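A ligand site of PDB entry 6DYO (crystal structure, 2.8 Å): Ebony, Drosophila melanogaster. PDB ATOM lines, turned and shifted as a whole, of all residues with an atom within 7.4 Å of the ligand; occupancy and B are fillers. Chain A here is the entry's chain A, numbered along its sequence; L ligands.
OE2 of Glu 32 is in hydrogen-bond range of O2 of the ligand, at 2.9 Å.
O of Phe 123 sits at hydrogen-bond distance from N1 of the ligand, at 3.5 Å.
The side-chain carboxylate of Glu 32 sits at hydrogen-bond distance from the side-chain hydroxyl of Tyr 44.
The side-chain hydroxyl (OG1) of Thr 162 lies within hydrogen-bond range of the side-chain carboxylate (OE2) of Glu 104 (3.0 Å).
The side-chain carboxylate of Glu 104 lies within hydrogen-bond range of a ring nitrogen (NE2) of His 121 (3.0 Å).
ND1 of His 121 is in hydrogen-bond range of OE2 of Glu 84, at 2.5 Å.
Merely in contact with the ligand: Thr 162, Val 96, Phe 25, Leu 100, Thr 164 and His 121.
Hydrophobic or aromatic side chains within 4 Å of the ligand: Phe 25, Val 96 and Leu 100.
Of the 24 residues printed, 8 come within 4 Å of the ligand.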
ATOM      1  N   PHE A  25     -28.328   8.216 -27.216  1.00  0.00           N
ATOM      2  CA  PHE A  25     -27.090   8.741 -26.660  1.00  0.00           C
ATOM      3  C   PHE A  25     -26.837  10.200 -27.029  1.00  0.00           C
ATOM      4  O   PHE A  25     -26.393  10.972 -26.179  1.00  0.00           O
ATOM      5  CB  PHE A  25     -25.903   7.896 -27.115  1.00  0.00           C
ATOM      6  CG  PHE A  25     -25.705   6.637 -26.315  1.00  0.00           C
ATOM      7  CD1 PHE A  25     -24.696   6.552 -25.362  1.00  0.00           C
ATOM      8  CD2 PHE A  25     -26.535   5.545 -26.507  1.00  0.00           C
ATOM      9  CE1 PHE A  25     -24.519   5.401 -24.626  1.00  0.00           C
ATOM     10  CE2 PHE A  25     -26.357   4.386 -25.760  1.00  0.00           C
ATOM     11  CZ  PHE A  25     -25.349   4.319 -24.820  1.00  0.00           C
ATOM     12  N   ALA A  29     -26.883  11.758 -23.393  1.00  0.00           N
ATOM     13  CA  ALA A  29     -25.890  11.092 -22.558  1.00  0.00           C
ATOM     14  C   ALA A  29     -25.349  12.058 -21.509  1.00  0.00           C
ATOM     15  O   ALA A  29     -24.939  13.173 -21.818  1.00  0.00           O
ATOM     16  CB  ALA A  29     -24.755  10.556 -23.416  1.00  0.00           C
ATOM     17  N   ASP A  30     -25.342  11.600 -20.252  1.00  0.00           N
ATOM     18  CA  ASP A  30     -24.992  12.474 -19.134  1.00  0.00           C
ATOM     19  C   ASP A  30     -23.537  12.911 -19.161  1.00  0.00           C
ATOM     20  O   ASP A  30     -23.189  13.900 -18.509  1.00  0.00           O
ATOM     21  CB  ASP A  30     -25.296  11.770 -17.812  1.00  0.00           C
ATOM     22  CG  ASP A  30     -26.785  11.529 -17.621  1.00  0.00           C
ATOM     23  OD1 ASP A  30     -27.378  10.777 -18.419  1.00  0.00           O
ATOM     24  OD2 ASP A  30     -27.355  12.091 -16.657  1.00  0.00           O
ATOM     25  N   LEU A  31     -22.676  12.215 -19.902  1.00  0.00           N
ATOM     26  CA  LEU A  31     -21.270  12.597 -19.977  1.00  0.00           C
ATOM     27  C   LEU A  31     -21.006  13.596 -21.106  1.00  0.00           C
ATOM     28  O   LEU A  31     -20.403  14.647 -20.876  1.00  0.00           O
ATOM     29  CB  LEU A  31     -20.392  11.357 -20.150  1.00  0.00           C
ATOM     30  CG  LEU A  31     -20.120  10.530 -18.894  1.00  0.00           C
ATOM     31  CD1 LEU A  31     -19.350   9.265 -19.241  1.00  0.00           C
ATOM     32  CD2 LEU A  31     -19.359  11.356 -17.863  1.00  0.00           C
ATOM     33  N   GLU A  32     -21.469  13.278 -22.320  1.00  0.00           N
ATOM     34  CA  GLU A  32     -21.134  14.089 -23.492  1.00  0.00           C
ATOM     35  C   GLU A  32     -21.749  15.482 -23.466  1.00  0.00           C
ATOM     36  O   GLU A  32     -21.347  16.324 -24.279  1.00  0.00           O
ATOM     37  CB  GLU A  32     -21.583  13.360 -24.761  1.00  0.00           C
ATOM     38  CG  GLU A  32     -20.838  12.064 -25.049  1.00  0.00           C
ATOM     39  CD  GLU A  32     -21.505  10.858 -24.403  1.00  0.00           C
ATOM     40  OE1 GLU A  32     -21.577  10.811 -23.161  1.00  0.00           O
ATOM     41  OE2 GLU A  32     -21.945   9.964 -25.154  1.00  0.00           O
ATOM     42  N   TYR A  44     -21.260   8.644 -32.932  1.00  0.00           N
ATOM     43  CA  TYR A  44     -21.678   7.328 -32.455  1.00  0.00           C
ATOM     44  C   TYR A  44     -21.791   6.333 -33.607  1.00  0.00           C
ATOM     45  O   TYR A  44     -21.337   5.192 -33.498  1.00  0.00           O
ATOM     46  CB  TYR A  44     -23.001   7.437 -31.702  1.00  0.00           C
ATOM     47  CG  TYR A  44     -22.985   8.396 -30.539  1.00  0.00           C
ATOM     48  CD1 TYR A  44     -22.319   8.077 -29.358  1.00  0.00           C
ATOM     49  CD2 TYR A  44     -23.634   9.620 -30.618  1.00  0.00           C
ATOM     50  CE1 TYR A  44     -22.292   8.954 -28.291  1.00  0.00           C
ATOM     51  CE2 TYR A  44     -23.618  10.507 -29.552  1.00  0.00           C
ATOM     52  CZ  TYR A  44     -22.951  10.164 -28.386  1.00  0.00           C
ATOM     53  OH  TYR A  44     -22.936  11.049 -27.330  1.00  0.00           O
ATOM     54  N   ILE A  47     -18.442   4.937 -34.699  1.00  0.00           N
ATOM     55  CA  ILE A  47     -17.942   3.857 -33.847  1.00  0.00           C
ATOM     56  C   ILE A  47     -18.733   2.578 -34.112  1.00  0.00           C
ATOM     57  O   ILE A  47     -18.159   1.484 -34.162  1.00  0.00           O
ATOM     58  CB  ILE A  47     -18.003   4.272 -32.368  1.00  0.00           C
ATOM     59  CG1 ILE A  47     -17.194   5.546 -32.133  1.00  0.00           C
ATOM     60  CG2 ILE A  47     -17.490   3.148 -31.487  1.00  0.00           C
ATOM     61  CD1 ILE A  47     -17.286   6.069 -30.718  1.00  0.00           C
ATOM     62  N   GLU A  84     -12.586  -7.288 -26.479  1.00  0.00           N
ATOM     63  CA  GLU A  84     -13.287  -6.207 -27.159  1.00  0.00           C
ATOM     64  C   GLU A  84     -12.450  -5.683 -28.319  1.00  0.00           C
ATOM     65  O   GLU A  84     -11.228  -5.552 -28.209  1.00  0.00           O
ATOM     66  CB  GLU A  84     -13.574  -5.067 -26.188  1.00  0.00           C
ATOM     67  CG  GLU A  84     -14.643  -5.370 -25.150  1.00  0.00           C
ATOM     68  CD  GLU A  84     -15.408  -4.129 -24.726  1.00  0.00           C
ATOM     69  OE1 GLU A  84     -14.881  -3.008 -24.908  1.00  0.00           O
ATOM     70  OE2 GLU A  84     -16.535  -4.271 -24.212  1.00  0.00           O
ATOM     71  N   LEU A  93     -15.452  11.831 -28.304  1.00  0.00           N
ATOM     72  CA  LEU A  93     -15.876  10.610 -27.623  1.00  0.00           C
ATOM     73  C   LEU A  93     -14.700   9.814 -27.084  1.00  0.00           C
ATOM     74  O   LEU A  93     -14.888   8.972 -26.207  1.00  0.00           O
ATOM     75  CB  LEU A  93     -16.700   9.746 -28.571  1.00  0.00           C
ATOM     76  CG  LEU A  93     -18.163  10.155 -28.759  1.00  0.00           C
ATOM     77  CD1 LEU A  93     -18.889   9.190 -29.689  1.00  0.00           C
ATOM     78  CD2 LEU A  93     -18.860  10.236 -27.409  1.00  0.00           C
ATOM     79  N   VAL A  96     -14.514  10.333 -23.446  1.00  0.00           N
ATOM     80  CA  VAL A  96     -15.474   9.511 -22.718  1.00  0.00           C
ATOM     81  C   VAL A  96     -14.938   8.092 -22.552  1.00  0.00           C
ATOM     82  O   VAL A  96     -15.002   7.509 -21.470  1.00  0.00           O
ATOM     83  CB  VAL A  96     -16.836   9.518 -23.426  1.00  0.00           C
ATOM     84  CG1 VAL A  96     -17.799   8.551 -22.749  1.00  0.00           C
ATOM     85  CG2 VAL A  96     -17.415  10.925 -23.445  1.00  0.00           C
ATOM     86  N   PHE A  97     -14.403   7.511 -23.634  1.00  0.00           N
ATOM     87  CA  PHE A  97     -13.925   6.137 -23.567  1.00  0.00           C
ATOM     88  C   PHE A  97     -12.649   6.016 -22.739  1.00  0.00           C
ATOM     89  O   PHE A  97     -12.435   4.980 -22.101  1.00  0.00           O
ATOM     90  CB  PHE A  97     -13.721   5.583 -24.980  1.00  0.00           C
ATOM     91  CG  PHE A  97     -14.997   5.109 -25.618  1.00  0.00           C
ATOM     92  CD1 PHE A  97     -15.365   3.768 -25.567  1.00  0.00           C
ATOM     93  CD2 PHE A  97     -15.834   6.000 -26.272  1.00  0.00           C
ATOM     94  CE1 PHE A  97     -16.540   3.335 -26.146  1.00  0.00           C
ATOM     95  CE2 PHE A  97     -17.009   5.568 -26.850  1.00  0.00           C
ATOM     96  CZ  PHE A  97     -17.368   4.239 -26.793  1.00  0.00           C
ATOM     97  N   LEU A 100     -13.989   5.987 -19.231  1.00  0.00           N
ATOM     98  CA  LEU A 100     -14.555   4.683 -18.884  1.00  0.00           C
ATOM     99  C   LEU A 100     -13.458   3.655 -18.630  1.00  0.00           C
ATOM    100  O   LEU A 100     -13.634   2.752 -17.802  1.00  0.00           O
ATOM    101  CB  LEU A 100     -15.493   4.209 -19.985  1.00  0.00           C
ATOM    102  CG  LEU A 100     -16.702   5.119 -20.220  1.00  0.00           C
ATOM    103  CD1 LEU A 100     -17.401   4.792 -21.535  1.00  0.00           C
ATOM    104  CD2 LEU A 100     -17.680   5.057 -19.053  1.00  0.00           C
ATOM    105  N   GLU A 104     -13.022   1.447 -15.461  1.00  0.00           N
ATOM    106  CA  GLU A 104     -13.083  -0.001 -15.635  1.00  0.00           C
ATOM    107  C   GLU A 104     -11.711  -0.675 -15.601  1.00  0.00           C
ATOM    108  O   GLU A 104     -11.632  -1.852 -15.235  1.00  0.00           O
ATOM    109  CB  GLU A 104     -13.771  -0.349 -16.957  1.00  0.00           C
ATOM    110  CG  GLU A 104     -15.273  -0.108 -16.953  1.00  0.00           C
ATOM    111  CD  GLU A 104     -15.857   0.027 -18.353  1.00  0.00           C
ATOM    112  OE1 GLU A 104     -15.091   0.284 -19.298  1.00  0.00           O
ATOM    113  OE2 GLU A 104     -17.089  -0.122 -18.500  1.00  0.00           O
ATOM    114  N   HIS A 121     -19.162  -7.743 -20.786  1.00  0.00           N
ATOM    115  CA  HIS A 121     -19.201  -6.297 -20.628  1.00  0.00           C
ATOM    116  C   HIS A 121     -20.439  -5.757 -21.335  1.00  0.00           C
ATOM    117  O   HIS A 121     -20.557  -5.855 -22.558  1.00  0.00           O
ATOM    118  CB  HIS A 121     -17.940  -5.640 -21.188  1.00  0.00           C
ATOM    119  CG  HIS A 121     -17.936  -4.153 -21.092  1.00  0.00           C
ATOM    120  ND1 HIS A 121     -17.243  -3.355 -21.978  1.00  0.00           N
ATOM    121  CD2 HIS A 121     -18.540  -3.305 -20.220  1.00  0.00           C
ATOM    122  CE1 HIS A 121     -17.413  -2.078 -21.656  1.00  0.00           C
ATOM    123  NE2 HIS A 121     -18.204  -2.025 -20.593  1.00  0.00           N
ATOM    124  N   SER A 122     -21.351  -5.179 -20.556  1.00  0.00           N
ATOM    125  CA  SER A 122     -22.512  -4.492 -21.133  1.00  0.00           C
ATOM    126  C   SER A 122     -22.000  -3.206 -21.780  1.00  0.00           C
ATOM    127  O   SER A 122     -21.721  -2.218 -21.105  1.00  0.00           O
ATOM    128  CB  SER A 122     -23.559  -4.201 -20.061  1.00  0.00           C
ATOM    129  OG  SER A 122     -24.677  -3.538 -20.624  1.00  0.00           O
ATOM    130  N   PHE A 123     -21.877  -3.236 -23.110  1.00  0.00           N
ATOM    131  CA  PHE A 123     -21.267  -2.145 -23.842  1.00  0.00           C
ATOM    132  C   PHE A 123     -22.228  -0.972 -24.000  1.00  0.00           C
ATOM    133  O   PHE A 123     -21.965   0.132 -23.492  1.00  0.00           O
ATOM    134  CB  PHE A 123     -20.782  -2.655 -25.203  1.00  0.00           C
ATOM    135  CG  PHE A 123     -20.187  -1.599 -26.091  1.00  0.00           C
ATOM    136  CD1 PHE A 123     -19.039  -0.927 -25.727  1.00  0.00           C
ATOM    137  CD2 PHE A 123     -20.762  -1.325 -27.327  1.00  0.00           C
ATOM    138  CE1 PHE A 123     -18.486   0.037 -26.552  1.00  0.00           C
ATOM    139  CE2 PHE A 123     -20.219  -0.364 -28.161  1.00  0.00           C
ATOM    140  CZ  PHE A 123     -19.081   0.321 -27.780  1.00  0.00           C
ATOM    141  N   MET A 124     -23.353  -1.186 -24.679  1.00  0.00           N
ATOM    142  CA  MET A 124     -24.330  -0.134 -24.912  1.00  0.00           C
ATOM    143  C   MET A 124     -25.740  -0.703 -24.797  1.00  0.00           C
ATOM    144  O   MET A 124     -25.964  -1.891 -25.041  1.00  0.00           O
ATOM    145  CB  MET A 124     -24.145   0.518 -26.290  1.00  0.00           C
ATOM    146  CG  MET A 124     -22.862   1.343 -26.406  1.00  0.00           C
ATOM    147  SD  MET A 124     -23.026   2.766 -27.508  1.00  0.00           S
ATOM    148  CE  MET A 124     -22.706   1.999 -29.094  1.00  0.00           C
ATOM    149  N   MET A 125     -26.673   0.164 -24.428  1.00  0.00           N
ATOM    150  CA  MET A 125     -28.091  -0.173 -24.332  1.00  0.00           C
ATOM    151  C   MET A 125     -28.917   1.022 -24.766  1.00  0.00           C
ATOM    152  O   MET A 125     -28.614   2.161 -24.401  1.00  0.00           O
ATOM    153  CB  MET A 125     -28.490  -0.588 -22.916  1.00  0.00           C
ATOM    154  CG  MET A 125     -28.680  -2.078 -22.717  1.00  0.00           C
ATOM    155  SD  MET A 125     -29.737  -2.410 -21.294  1.00  0.00           S
ATOM    156  CE  MET A 125     -29.200  -4.070 -20.860  1.00  0.00           C
ATOM    157  N   PHE A 160     -20.733  -6.864 -16.310  1.00  0.00           N
ATOM    158  CA  PHE A 160     -19.860  -5.778 -15.872  1.00  0.00           C
ATOM    159  C   PHE A 160     -20.070  -4.575 -16.782  1.00  0.00           C
ATOM    160  O   PHE A 160     -20.034  -4.723 -18.011  1.00  0.00           O
ATOM    161  CB  PHE A 160     -18.405  -6.257 -15.915  1.00  0.00           C
ATOM    162  CG  PHE A 160     -17.394  -5.212 -15.577  1.00  0.00           C
ATOM    163  CD1 PHE A 160     -17.268  -4.739 -14.281  1.00  0.00           C
ATOM    164  CD2 PHE A 160     -16.523  -4.745 -16.541  1.00  0.00           C
ATOM    165  CE1 PHE A 160     -16.312  -3.794 -13.960  1.00  0.00           C
ATOM    166  CE2 PHE A 160     -15.568  -3.793 -16.231  1.00  0.00           C
ATOM    167  CZ  PHE A 160     -15.461  -3.321 -14.935  1.00  0.00           C
ATOM    168  N   THR A 161     -20.309  -3.411 -16.197  1.00  0.00           N
ATOM    169  CA  THR A 161     -20.502  -2.199 -16.976  1.00  0.00           C
ATOM    170  C   THR A 161     -20.348  -0.968 -16.083  1.00  0.00           C
ATOM    171  O   THR A 161     -20.307  -1.070 -14.854  1.00  0.00           O
ATOM    172  CB  THR A 161     -21.875  -2.169 -17.669  1.00  0.00           C
ATOM    173  OG1 THR A 161     -21.866  -1.192 -18.712  1.00  0.00           O
ATOM    174  CG2 THR A 161     -22.971  -1.815 -16.670  1.00  0.00           C
ATOM    175  N   THR A 162     -20.260   0.192 -16.728  1.00  0.00           N
ATOM    176  CA  THR A 162     -20.211   1.479 -16.058  1.00  0.00           C
ATOM    177  C   THR A 162     -21.494   2.228 -16.398  1.00  0.00           C
ATOM    178  O   THR A 162     -21.774   2.487 -17.571  1.00  0.00           O
ATOM    179  CB  THR A 162     -18.984   2.294 -16.487  1.00  0.00           C
ATOM    180  OG1 THR A 162     -17.793   1.585 -16.121  1.00  0.00           O
ATOM    181  CG2 THR A 162     -18.980   3.651 -15.809  1.00  0.00           C
ATOM    182  N   ASN A 163     -22.267   2.582 -15.371  1.00  0.00           N
ATOM    183  CA  ASN A 163     -23.546   3.241 -15.559  1.00  0.00           C
ATOM    184  C   ASN A 163     -23.393   4.738 -15.286  1.00  0.00           C
ATOM    185  O   ASN A 163     -22.951   5.129 -14.200  1.00  0.00           O
ATOM    186  CB  ASN A 163     -24.611   2.613 -14.654  1.00  0.00           C
ATOM    187  CG  ASN A 163     -25.100   1.282 -15.176  1.00  0.00           C
ATOM    188  OD1 ASN A 163     -25.373   1.137 -16.373  1.00  0.00           O
ATOM    189  ND2 ASN A 163     -25.198   0.303 -14.303  1.00  0.00           N
ATOM    190  N   THR A 164     -23.770   5.553 -16.269  1.00  0.00           N
ATOM    191  CA  THR A 164     -23.544   6.985 -16.231  1.00  0.00           C
ATOM    192  C   THR A 164     -24.831   7.800 -16.166  1.00  0.00           C
ATOM    193  O   THR A 164     -24.766   9.021 -16.045  1.00  0.00           O
ATOM    194  CB  THR A 164     -22.715   7.424 -17.454  1.00  0.00           C
ATOM    195  OG1 THR A 164     -23.416   7.070 -18.651  1.00  0.00           O
ATOM    196  CG2 THR A 164     -21.353   6.742 -17.449  1.00  0.00           C
ATOM    197  N   SER A 165     -25.985   7.148 -16.246  1.00  0.00           N
ATOM    198  CA  SER A 165     -27.258   7.841 -16.083  1.00  0.00           C
ATOM    199  C   SER A 165     -27.924   7.423 -14.779  1.00  0.00           C
ATOM    200  O   SER A 165     -27.723   6.297 -14.316  1.00  0.00           O
ATOM    201  CB  SER A 165     -28.214   7.567 -17.247  1.00  0.00           C
ATOM    202  OG  SER A 165     -29.088   6.499 -16.930  1.00  0.00           O
HETATM  203  C1  LIG L   1     -21.718   3.050 -21.321  1.00  0.00           C
HETATM  204  C2  LIG L   1     -21.384   4.236 -22.227  1.00  0.00           C
HETATM  205  C3  LIG L   1     -20.763   6.396 -23.858  1.00  0.00           C
HETATM  206  C4  LIG L   1     -21.772   5.516 -21.856  1.00  0.00           C
HETATM  207  C5  LIG L   1     -20.680   4.037 -23.409  1.00  0.00           C
HETATM  208  C6  LIG L   1     -20.374   5.119 -24.219  1.00  0.00           C
HETATM  209  C7  LIG L   1     -21.467   6.595 -22.676  1.00  0.00           C
HETATM  210  O1  LIG L   1     -21.866   7.886 -22.298  1.00  0.00           O
HETATM  211  O2  LIG L   1     -20.458   7.485 -24.680  1.00  0.00           O
HETATM  212  C8  LIG L   1     -20.485   2.666 -20.505  1.00  0.00           C
HETATM  213  N1  LIG L   1     -19.809   1.540 -21.125  1.00  0.00           N
